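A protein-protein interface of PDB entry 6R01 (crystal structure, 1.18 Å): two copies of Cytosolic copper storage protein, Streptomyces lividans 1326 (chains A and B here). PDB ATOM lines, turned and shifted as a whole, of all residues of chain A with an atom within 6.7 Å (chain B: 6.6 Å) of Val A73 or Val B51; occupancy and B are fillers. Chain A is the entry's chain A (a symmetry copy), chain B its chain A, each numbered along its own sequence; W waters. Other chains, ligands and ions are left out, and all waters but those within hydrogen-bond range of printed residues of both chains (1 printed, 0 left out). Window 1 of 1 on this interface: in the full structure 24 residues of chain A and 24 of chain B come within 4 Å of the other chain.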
ATOM      1  N   VAL A  51     -19.606  -2.275  -0.044  1.00  0.00           N
ATOM      2  CA  VAL A  51     -20.116  -1.546   1.154  1.00  0.00           C
ATOM      3  C   VAL A  51     -20.150  -2.484   2.360  1.00  0.00           C
ATOM      4  O   VAL A  51     -19.755  -2.060   3.442  1.00  0.00           O
ATOM      5  CB  VAL A  51     -21.492  -0.904   0.870  1.00  0.00           C
ATOM      6  CG1 VAL A  51     -22.104  -0.273   2.124  1.00  0.00           C
ATOM      7  CG2 VAL A  51     -21.399   0.131  -0.237  1.00  0.00           C
ATOM      8  N   ALA A  54     -16.583  -2.702   3.744  1.00  0.00           N
ATOM      9  CA  ALA A  54     -16.188  -1.494   4.494  1.00  0.00           C
ATOM     10  C   ALA A  54     -16.921  -1.472   5.848  1.00  0.00           C
ATOM     11  O   ALA A  54     -16.304  -1.149   6.864  1.00  0.00           O
ATOM     12  CB  ALA A  54     -16.542  -0.263   3.704  1.00  0.00           C
ATOM     13  N   THR A  55     -18.200  -1.855   5.848  1.00  0.00           N
ATOM     14  CA  THR A  55     -19.036  -1.799   7.074  1.00  0.00           C
ATOM     15  C   THR A  55     -18.498  -2.809   8.084  1.00  0.00           C
ATOM     16  O   THR A  55     -18.395  -2.506   9.262  1.00  0.00           O
ATOM     17  CB  THR A  55     -20.495  -2.046   6.710  1.00  0.00           C
ATOM     18  OG1 THR A  55     -20.924  -1.028   5.803  1.00  0.00           O
ATOM     19  CG2 THR A  55     -21.393  -1.972   7.928  1.00  0.00           C
ATOM     20  N   ALA A  56     -18.152  -4.025   7.645  1.00  0.00           N
ATOM     21  CA  ALA A  56     -17.607  -5.046   8.563  1.00  0.00           C
ATOM     22  C   ALA A  56     -16.375  -4.478   9.258  1.00  0.00           C
ATOM     23  O   ALA A  56     -16.175  -4.728  10.454  1.00  0.00           O
ATOM     24  CB  ALA A  56     -17.266  -6.303   7.809  1.00  0.00           C
ATOM     25  N   VAL A  58     -15.360  -1.166   9.657  1.00  0.00           N
ATOM     26  CA  VAL A  58     -15.658  -0.044  10.579  1.00  0.00           C
ATOM     27  C   VAL A  58     -16.282  -0.590  11.867  1.00  0.00           C
ATOM     28  O   VAL A  58     -15.927  -0.082  12.943  1.00  0.00           O
ATOM     29  CB  VAL A  58     -16.567   0.970   9.874  1.00  0.00           C
ATOM     30  CG1 VAL A  58     -17.112   1.988  10.842  1.00  0.00           C
ATOM     31  CG2 VAL A  58     -15.849   1.663   8.731  1.00  0.00           C
ATOM     32  N   LEU A  59     -17.203  -1.553  11.783  1.00  0.00           N
ATOM     33  CA  LEU A  59     -17.958  -2.015  12.984  1.00  0.00           C
ATOM     34  C   LEU A  59     -17.032  -2.867  13.855  1.00  0.00           C
ATOM     35  O   LEU A  59     -17.324  -3.010  15.046  1.00  0.00           O
ATOM     36  CB  LEU A  59     -19.196  -2.800  12.555  1.00  0.00           C
ATOM     37  CG  LEU A  59     -20.464  -1.989  12.316  1.00  0.00           C
ATOM     38  CD1 LEU A  59     -21.137  -1.666  13.642  1.00  0.00           C
ATOM     39  CD2 LEU A  59     -20.205  -0.706  11.542  1.00  0.00           C
ATOM     40  N   ASN A  68     -21.714   8.858  15.028  1.00  0.00           N
ATOM     41  CA  ASN A  68     -22.113   9.559  13.774  1.00  0.00           C
ATOM     42  C   ASN A  68     -21.574   8.789  12.576  1.00  0.00           C
ATOM     43  O   ASN A  68     -22.332   8.557  11.612  1.00  0.00           O
ATOM     44  CB  ASN A  68     -21.633  11.016  13.704  1.00  0.00           C
ATOM     45  CG  ASN A  68     -22.227  11.893  14.774  1.00  0.00           C
ATOM     46  OD1 ASN A  68     -23.359  11.670  15.190  1.00  0.00           O
ATOM     47  ND2 ASN A  68     -21.473  12.891  15.205  1.00  0.00           N
ATOM     48  N   VAL A  69     -20.302   8.407  12.650  1.00  0.00           N
ATOM     49  CA  VAL A  69     -19.649   7.638  11.559  1.00  0.00           C
ATOM     50  C   VAL A  69     -20.353   6.282  11.467  1.00  0.00           C
ATOM     51  O   VAL A  69     -20.789   5.891  10.373  1.00  0.00           O
ATOM     52  CB  VAL A  69     -18.134   7.508  11.794  1.00  0.00           C
ATOM     53  CG1 VAL A  69     -17.484   6.498  10.854  1.00  0.00           C
ATOM     54  CG2 VAL A  69     -17.453   8.861  11.691  1.00  0.00           C
ATOM     55  N   THR A  70     -20.490   5.594  12.590  1.00  0.00           N
ATOM     56  CA  THR A  70     -21.031   4.213  12.599  1.00  0.00           C
ATOM     57  C   THR A  70     -22.468   4.233  12.069  1.00  0.00           C
ATOM     58  O   THR A  70     -22.819   3.388  11.264  1.00  0.00           O
ATOM     59  CB  THR A  70     -20.928   3.596  13.993  1.00  0.00           C
ATOM     60  OG1 THR A  70     -19.541   3.563  14.317  1.00  0.00           O
ATOM     61  CG2 THR A  70     -21.560   2.231  14.063  1.00  0.00           C
ATOM     62  N   ARG A  71     -23.294   5.175  12.523  1.00  0.00           N
ATOM     63  CA  ARG A  71     -24.693   5.298  12.044  1.00  0.00           C
ATOM     64  C   ARG A  71     -24.716   5.485  10.519  1.00  0.00           C
ATOM     65  O   ARG A  71     -25.488   4.784   9.853  1.00  0.00           O
ATOM     66  CB  ARG A  71     -25.433   6.445  12.750  1.00  0.00           C
ATOM     67  CG  ARG A  71     -26.060   6.074  14.086  1.00  0.00           C
ATOM     68  CD  ARG A  71     -27.059   7.127  14.535  1.00  0.00           C
ATOM     69  NE  ARG A  71     -26.430   8.437  14.633  1.00  0.00           N
ATOM     70  CZ  ARG A  71     -25.959   8.983  15.754  1.00  0.00           C
ATOM     71  NH1 ARG A  71     -26.052   8.347  16.912  1.00  0.00           N
ATOM     72  NH2 ARG A  71     -25.387  10.173  15.711  1.00  0.00           N
ATOM     73  N   ALA A  72     -23.916   6.401   9.977  1.00  0.00           N
ATOM     74  CA  ALA A  72     -23.956   6.750   8.537  1.00  0.00           C
ATOM     75  C   ALA A  72     -23.501   5.537   7.703  1.00  0.00           C
ATOM     76  O   ALA A  72     -24.095   5.252   6.681  1.00  0.00           O
ATOM     77  CB  ALA A  72     -23.120   7.980   8.284  1.00  0.00           C
ATOM     78  N   VAL A  73     -22.508   4.815   8.193  1.00  0.00           N
ATOM     79  CA  VAL A  73     -21.998   3.604   7.487  1.00  0.00           C
ATOM     80  C   VAL A  73     -23.067   2.501   7.566  1.00  0.00           C
ATOM     81  O   VAL A  73     -23.372   1.913   6.540  1.00  0.00           O
ATOM     82  CB  VAL A  73     -20.660   3.178   8.090  1.00  0.00           C
ATOM     83  CG1 VAL A  73     -20.287   1.818   7.578  1.00  0.00           C
ATOM     84  CG2 VAL A  73     -19.550   4.178   7.821  1.00  0.00           C
ATOM     85  N   LEU A  74     -23.703   2.276   8.730  1.00  0.00           N
ATOM     86  CA  LEU A  74     -24.770   1.247   8.811  1.00  0.00           C
ATOM     87  C   LEU A  74     -25.919   1.641   7.882  1.00  0.00           C
ATOM     88  O   LEU A  74     -26.542   0.747   7.285  1.00  0.00           O
ATOM     89  CB  LEU A  74     -25.299   1.101  10.241  1.00  0.00           C
ATOM     90  CG  LEU A  74     -24.337   0.436  11.215  1.00  0.00           C
ATOM     91  CD1 LEU A  74     -24.818   0.540  12.646  1.00  0.00           C
ATOM     92  CD2 LEU A  74     -24.109  -1.019  10.838  1.00  0.00           C
ATOM     93  N   GLN A  75     -26.277   2.927   7.852  1.00  0.00           N
ATOM     94  CA  GLN A  75     -27.376   3.342   6.946  1.00  0.00           C
ATOM     95  C   GLN A  75     -27.007   2.979   5.483  1.00  0.00           C
ATOM     96  O   GLN A  75     -27.849   2.303   4.728  1.00  0.00           O
ATOM     97  CB  GLN A  75     -27.693   4.826   7.052  1.00  0.00           C
ATOM     98  CG  GLN A  75     -28.881   5.175   6.168  1.00  0.00           C
ATOM     99  CD  GLN A  75     -30.124   4.398   6.550  1.00  0.00           C
ATOM    100  OE1 GLN A  75     -30.672   3.614   5.761  1.00  0.00           O
ATOM    101  NE2 GLN A  75     -30.584   4.599   7.780  1.00  0.00           N
ATOM    102  N   ALA A  76     -25.755   3.313   5.082  1.00  0.00           N
ATOM    103  CA  ALA A  76     -25.363   3.036   3.683  1.00  0.00           C
ATOM    104  C   ALA A  76     -25.490   1.523   3.430  1.00  0.00           C
ATOM    105  O   ALA A  76     -26.004   1.101   2.402  1.00  0.00           O
ATOM    106  CB  ALA A  76     -23.970   3.521   3.410  1.00  0.00           C
ATOM    107  N   CYS A  77     -25.073   0.722   4.397  1.00  0.00           N
ATOM    108  CA  CYS A  77     -25.048  -0.743   4.188  1.00  0.00           C
ATOM    109  C   CYS A  77     -26.474  -1.291   4.150  1.00  0.00           C
ATOM    110  O   CYS A  77     -26.786  -2.217   3.405  1.00  0.00           O
ATOM    111  CB  CYS A  77     -24.286  -1.492   5.255  1.00  0.00           C
ATOM    112  SG  CYS A  77     -23.658  -3.038   4.549  1.00  0.00           S
ATOM    113  N   ALA A  78     -27.342  -0.760   5.021  1.00  0.00           N
ATOM    114  CA  ALA A  78     -28.766  -1.174   5.013  1.00  0.00           C
ATOM    115  C   ALA A  78     -29.346  -0.901   3.596  1.00  0.00           C
ATOM    116  O   ALA A  78     -29.873  -1.886   2.921  1.00  0.00           O
ATOM    117  CB  ALA A  78     -29.584  -0.436   6.085  1.00  0.00           C
ATOM    118  N   CYS A 112     -28.182  -4.755  10.030  1.00  0.00           N
ATOM    119  CA  CYS A 112     -27.805  -3.317  10.031  1.00  0.00           C
ATOM    120  C   CYS A 112     -28.942  -2.485  10.669  1.00  0.00           C
ATOM    121  O   CYS A 112     -28.660  -1.607  11.519  1.00  0.00           O
ATOM    122  CB  CYS A 112     -27.510  -2.828   8.617  1.00  0.00           C
ATOM    123  SG  CYS A 112     -25.949  -3.465   7.933  1.00  0.00           S
ATOM    124  N   LEU A 116     -28.824  -0.232  13.996  1.00  0.00           N
ATOM    125  CA  LEU A 116     -29.127   1.197  13.734  1.00  0.00           C
ATOM    126  C   LEU A 116     -30.132   1.661  14.776  1.00  0.00           C
ATOM    127  O   LEU A 116     -29.957   2.765  15.349  1.00  0.00           O
ATOM    128  CB  LEU A 116     -29.726   1.325  12.328  1.00  0.00           C
ATOM    129  CG  LEU A 116     -29.376   2.577  11.529  1.00  0.00           C
ATOM    130  CD1 LEU A 116     -27.996   3.111  11.868  1.00  0.00           C
ATOM    131  CD2 LEU A 116     -29.471   2.282  10.042  1.00  0.00           C
ATOM    132  N   CYS B  15     -11.774  10.637  -3.495  1.00  0.00           N
ATOM    133  CA  CYS B  15     -11.906   9.436  -2.631  1.00  0.00           C
ATOM    134  C   CYS B  15     -10.594   8.629  -2.704  1.00  0.00           C
ATOM    135  O   CYS B  15     -10.105   8.175  -1.663  1.00  0.00           O
ATOM    136  CB  CYS B  15     -13.064   8.527  -3.026  1.00  0.00           C
ATOM    137  SG  CYS B  15     -14.714   9.090  -2.518  1.00  0.00           S
ATOM    138  N   ALA B  19      -8.323   8.173   0.493  1.00  0.00           N
ATOM    139  CA  ALA B  19      -8.099   6.801   1.025  1.00  0.00           C
ATOM    140  C   ALA B  19      -6.596   6.555   1.218  1.00  0.00           C
ATOM    141  O   ALA B  19      -6.175   6.148   2.327  1.00  0.00           O
ATOM    142  CB  ALA B  19      -8.727   5.775   0.133  1.00  0.00           C
ATOM    143  N   MET B  46      -8.225   4.680   9.490  1.00  0.00           N
ATOM    144  CA  MET B  46      -8.565   3.328   8.976  1.00  0.00           C
ATOM    145  C   MET B  46      -9.997   3.334   8.430  1.00  0.00           C
ATOM    146  O   MET B  46     -10.230   2.859   7.289  1.00  0.00           O
ATOM    147  CB  MET B  46      -8.468   2.238  10.047  1.00  0.00           C
ATOM    148  CG  MET B  46      -7.083   2.025  10.657  1.00  0.00           C
ATOM    149  SD  MET B  46      -7.162   0.902  12.116  1.00  0.00           S
ATOM    150  CE  MET B  46      -5.449   0.660  12.558  1.00  0.00           C
ATOM    151  N   ASP B  47     -10.931   3.907   9.196  1.00  0.00           N
ATOM    152  CA  ASP B  47     -12.333   3.907   8.716  1.00  0.00           C
ATOM    153  C   ASP B  47     -12.415   4.755   7.451  1.00  0.00           C
ATOM    154  O   ASP B  47     -13.118   4.421   6.504  1.00  0.00           O
ATOM    155  CB  ASP B  47     -13.247   4.524   9.762  1.00  0.00           C
ATOM    156  CG  ASP B  47     -13.533   3.686  10.989  1.00  0.00           C
ATOM    157  OD1 ASP B  47     -13.272   2.467  10.997  1.00  0.00           O
ATOM    158  OD2 ASP B  47     -14.058   4.288  11.939  1.00  0.00           O
ATOM    159  N   CYS B  48     -11.769   5.904   7.508  1.00  0.00           N
ATOM    160  CA  CYS B  48     -11.888   6.863   6.401  1.00  0.00           C
ATOM    161  C   CYS B  48     -11.318   6.257   5.114  1.00  0.00           C
ATOM    162  O   CYS B  48     -11.894   6.534   4.031  1.00  0.00           O
ATOM    163  CB  CYS B  48     -11.210   8.170   6.760  1.00  0.00           C
ATOM    164  SG  CYS B  48     -11.878   9.550   5.812  1.00  0.00           S
ATOM    165  N   ALA B  49     -10.242   5.472   5.223  1.00  0.00           N
ATOM    166  CA  ALA B  49      -9.695   4.809   4.038  1.00  0.00           C
ATOM    167  C   ALA B  49     -10.701   3.778   3.530  1.00  0.00           C
ATOM    168  O   ALA B  49     -10.898   3.731   2.306  1.00  0.00           O
ATOM    169  CB  ALA B  49      -8.370   4.161   4.344  1.00  0.00           C
ATOM    170  N   ASP B  50     -11.272   2.962   4.412  1.00  0.00           N
ATOM    171  CA  ASP B  50     -12.193   1.875   3.989  1.00  0.00           C
ATOM    172  C   ASP B  50     -13.388   2.504   3.262  1.00  0.00           C
ATOM    173  O   ASP B  50     -13.852   2.021   2.243  1.00  0.00           O
ATOM    174  CB  ASP B  50     -12.607   1.012   5.176  1.00  0.00           C
ATOM    175  CG  ASP B  50     -11.469   0.160   5.691  1.00  0.00           C
ATOM    176  OD1 ASP B  50     -10.547  -0.118   4.907  1.00  0.00           O
ATOM    177  OD2 ASP B  50     -11.524  -0.189   6.855  1.00  0.00           O
ATOM    178  N   VAL B  51     -13.919   3.596   3.809  1.00  0.00           N
ATOM    179  CA  VAL B  51     -15.179   4.164   3.248  1.00  0.00           C
ATOM    180  C   VAL B  51     -14.881   4.909   1.947  1.00  0.00           C
ATOM    181  O   VAL B  51     -15.641   4.752   0.996  1.00  0.00           O
ATOM    182  CB  VAL B  51     -15.897   5.056   4.284  1.00  0.00           C
ATOM    183  CG1 VAL B  51     -17.115   5.767   3.688  1.00  0.00           C
ATOM    184  CG2 VAL B  51     -16.311   4.257   5.506  1.00  0.00           C
ATOM    185  N   CYS B  52     -13.760   5.630   1.882  1.00  0.00           N
ATOM    186  CA  CYS B  52     -13.398   6.326   0.622  1.00  0.00           C
ATOM    187  C   CYS B  52     -13.162   5.279  -0.469  1.00  0.00           C
ATOM    188  O   CYS B  52     -13.526   5.501  -1.601  1.00  0.00           O
ATOM    189  CB  CYS B  52     -12.166   7.206   0.770  1.00  0.00           C
ATOM    190  SG  CYS B  52     -12.543   8.739   1.635  1.00  0.00           S
ATOM    191  N   THR B  53     -12.511   4.156  -0.133  1.00  0.00           N
ATOM    192  CA  THR B  53     -12.273   3.087  -1.136  1.00  0.00           C
ATOM    193  C   THR B  53     -13.600   2.558  -1.704  1.00  0.00           C
ATOM    194  O   THR B  53     -13.765   2.473  -2.924  1.00  0.00           O
ATOM    195  CB  THR B  53     -11.462   1.954  -0.493  1.00  0.00           C
ATOM    196  OG1 THR B  53     -10.164   2.469  -0.184  1.00  0.00           O
ATOM    197  CG2 THR B  53     -11.295   0.763  -1.408  1.00  0.00           C
ATOM    198  N   ALA B  54     -14.571   2.285  -0.830  1.00  0.00           N
ATOM    199  CA  ALA B  54     -15.879   1.746  -1.252  1.00  0.00           C
ATOM    200  C   ALA B  54     -16.629   2.811  -2.074  1.00  0.00           C
ATOM    201  O   ALA B  54     -17.227   2.474  -3.096  1.00  0.00           O
ATOM    202  CB  ALA B  54     -16.692   1.370  -0.043  1.00  0.00           C
ATOM    203  N   THR B  55     -16.548   4.072  -1.644  1.00  0.00           N
ATOM    204  CA  THR B  55     -17.293   5.175  -2.301  1.00  0.00           C
ATOM    205  C   THR B  55     -16.732   5.380  -3.706  1.00  0.00           C
ATOM    206  O   THR B  55     -17.487   5.554  -4.650  1.00  0.00           O
ATOM    207  CB  THR B  55     -17.211   6.431  -1.442  1.00  0.00           C
ATOM    208  OG1 THR B  55     -17.802   6.160  -0.169  1.00  0.00           O
ATOM    209  CG2 THR B  55     -17.981   7.580  -2.061  1.00  0.00           C
ATOM    210  N   ALA B  56     -15.404   5.368  -3.868  1.00  0.00           N
ATOM    211  CA  ALA B  56     -14.793   5.542  -5.201  1.00  0.00           C
ATOM    212  C   ALA B  56     -15.345   4.476  -6.140  1.00  0.00           C
ATOM    213  O   ALA B  56     -15.601   4.767  -7.317  1.00  0.00           O
ATOM    214  CB  ALA B  56     -13.293   5.450  -5.109  1.00  0.00           C
ATOM    215  N   ALA B  72     -26.736   7.472  -0.058  1.00  0.00           N
ATOM    216  CA  ALA B  72     -26.430   6.928   1.286  1.00  0.00           C
ATOM    217  C   ALA B  72     -24.912   6.695   1.412  1.00  0.00           C
ATOM    218  O   ALA B  72     -24.340   6.996   2.442  1.00  0.00           O
ATOM    219  CB  ALA B  72     -27.236   5.676   1.529  1.00  0.00           C
ATOM    220  N   VAL B  73     -24.289   6.233   0.341  1.00  0.00           N
ATOM    221  CA  VAL B  73     -22.817   5.992   0.335  1.00  0.00           C
ATOM    222  C   VAL B  73     -22.096   7.349   0.381  1.00  0.00           C
ATOM    223  O   VAL B  73     -21.197   7.502   1.193  1.00  0.00           O
ATOM    224  CB  VAL B  73     -22.435   5.157  -0.886  1.00  0.00           C
ATOM    225  CG1 VAL B  73     -20.943   5.150  -1.044  1.00  0.00           C
ATOM    226  CG2 VAL B  73     -22.977   3.740  -0.822  1.00  0.00           C
ATOM    227  N   ALA B  76     -22.277   8.640   3.895  1.00  0.00           N
ATOM    228  CA  ALA B  76     -21.352   7.952   4.821  1.00  0.00           C
ATOM    229  C   ALA B  76     -19.937   8.521   4.612  1.00  0.00           C
ATOM    230  O   ALA B  76     -19.226   8.797   5.569  1.00  0.00           O
ATOM    231  CB  ALA B  76     -21.381   6.467   4.604  1.00  0.00           C
ATOM    232  N   CYS B  77     -19.566   8.744   3.361  1.00  0.00           N
ATOM    233  CA  CYS B  77     -18.182   9.176   3.064  1.00  0.00           C
ATOM    234  C   CYS B  77     -17.970  10.614   3.538  1.00  0.00           C
ATOM    235  O   CYS B  77     -16.895  10.982   4.010  1.00  0.00           O
ATOM    236  CB  CYS B  77     -17.831   9.109   1.598  1.00  0.00           C
ATOM    237  SG  CYS B  77     -16.040   8.883   1.434  1.00  0.00           S
ATOM    238  N   ALA B  78     -18.986  11.464   3.344  1.00  0.00           N
ATOM    239  CA  ALA B  78     -18.904  12.861   3.834  1.00  0.00           C
ATOM    240  C   ALA B  78     -18.649  12.826   5.368  1.00  0.00           C
ATOM    241  O   ALA B  78     -17.597  13.427   5.854  1.00  0.00           O
ATOM    242  CB  ALA B  78     -20.179  13.657   3.514  1.00  0.00           C
ATOM    243  N   THR B  79     -19.538  12.019   6.042  1.00  0.00           N
ATOM    244  CA  THR B  79     -19.536  11.988   7.542  1.00  0.00           C
ATOM    245  C   THR B  79     -18.156  11.528   8.074  1.00  0.00           C
ATOM    246  O   THR B  79     -17.619  12.083   9.068  1.00  0.00           O
ATOM    247  CB  THR B  79     -20.710  11.140   8.063  1.00  0.00           C
ATOM    248  OG1 THR B  79     -21.893  11.791   7.603  1.00  0.00           O
ATOM    249  CG2 THR B  79     -20.708  11.002   9.571  1.00  0.00           C
ATOM    250  N   VAL B  80     -17.567  10.496   7.418  1.00  0.00           N
ATOM    251  CA  VAL B  80     -16.284   9.981   7.956  1.00  0.00           C
ATOM    252  C   VAL B  80     -15.161  10.958   7.572  1.00  0.00           C
ATOM    253  O   VAL B  80     -14.294  11.193   8.415  1.00  0.00           O
ATOM    254  CB  VAL B  80     -16.003   8.534   7.526  1.00  0.00           C
ATOM    255  CG1 VAL B  80     -15.774   8.437   6.040  1.00  0.00           C
ATOM    256  CG2 VAL B  80     -14.828   7.980   8.304  1.00  0.00           C
HETATM  257  O   HOH W   1     -25.375   6.972   4.977  1.00  0.00           O
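Of the printed residues of chain B, Val A51 touches Val B73. Printed residues of chain B within 4 Å of Ala A54: Asp B50 (3.8 Å). Of the printed residues of chain B, Val A73 touches Val B51 (3.98 Å). Leu A74 touches none of the printed residues of chain B. Printed residues of chain A within 4 Å of Val B51: Val A73 (3.98 Å). Cys B52 touches none of the printed residues of chain A. Of the printed residues of chain A, Thr B79 touches Asn A68 and Ala A72. The nearest printed residue of chain A that does not touch Val B51 is Val A58 (4.2 Å).
Water W1 bridges the backbone carbonyl oxygen of Ala B72 (2.7 Å) and the backbone carbonyl oxygen of Ala A72 (2.7 Å).
Among the printed residues, merely in contact across the chains: Val A51 with Val B73, Ala A54 with Asp B50, Val A58 with Asp B47, Asn A68 with Thr B79, Val A69 with Val B80, Ala A72 with Ala B76, Ala A72 with Thr B79, Val A73 with Val B51 and Ala A76 with Ala B72.
The backbone carbonyl oxygen (O) of Val B51 is in hydrogen-bond range of the side-chain hydroxyl (OG1) of Thr B55 (2.8 Å). O of Val A51 is in hydrogen-bond range of OG1 of Thr A55, 2.8 Å away. NH2 of Arg A71 is in hydrogen-bond range of OD1 of Asn A68, at 2.6 Å.
Val A51 touches Val B73, and with the chains exchanged Val A73 touches Val B51. Ala A72 touches Ala B76, and with the chains exchanged Ala A76 touches Ala B72. Positions printed for both chains: 51, 54, 55, 56, 72, 73, 76, 77 and 78.
Of the 20 printed residues of chain B, 8 touch a printed residue of chain A. Printed residues of chain B that touch a printed residue of chain A: Asp B47, Asp B50, Val B51, Ala B72, Val B73, Ala B76, Thr B79 and Val B80. Printed residues of chain A that touch a printed residue of chain B: Val A51, Ala A54, Val A58, Asn A68, Val A69, Ala A72, Val A73 and Ala A76. Hydrophobic or aromatic side chains of chain A within 4 Å of the printed part of chain B: Val A51, Ala A54, Val A58, Val A69, Ala A72, Val A73 and Ala A76. Among the printed residues, no Asp or Glu carboxylate lies within 4 Å of a Lys or Arg side-chain nitrogen of the other chain.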
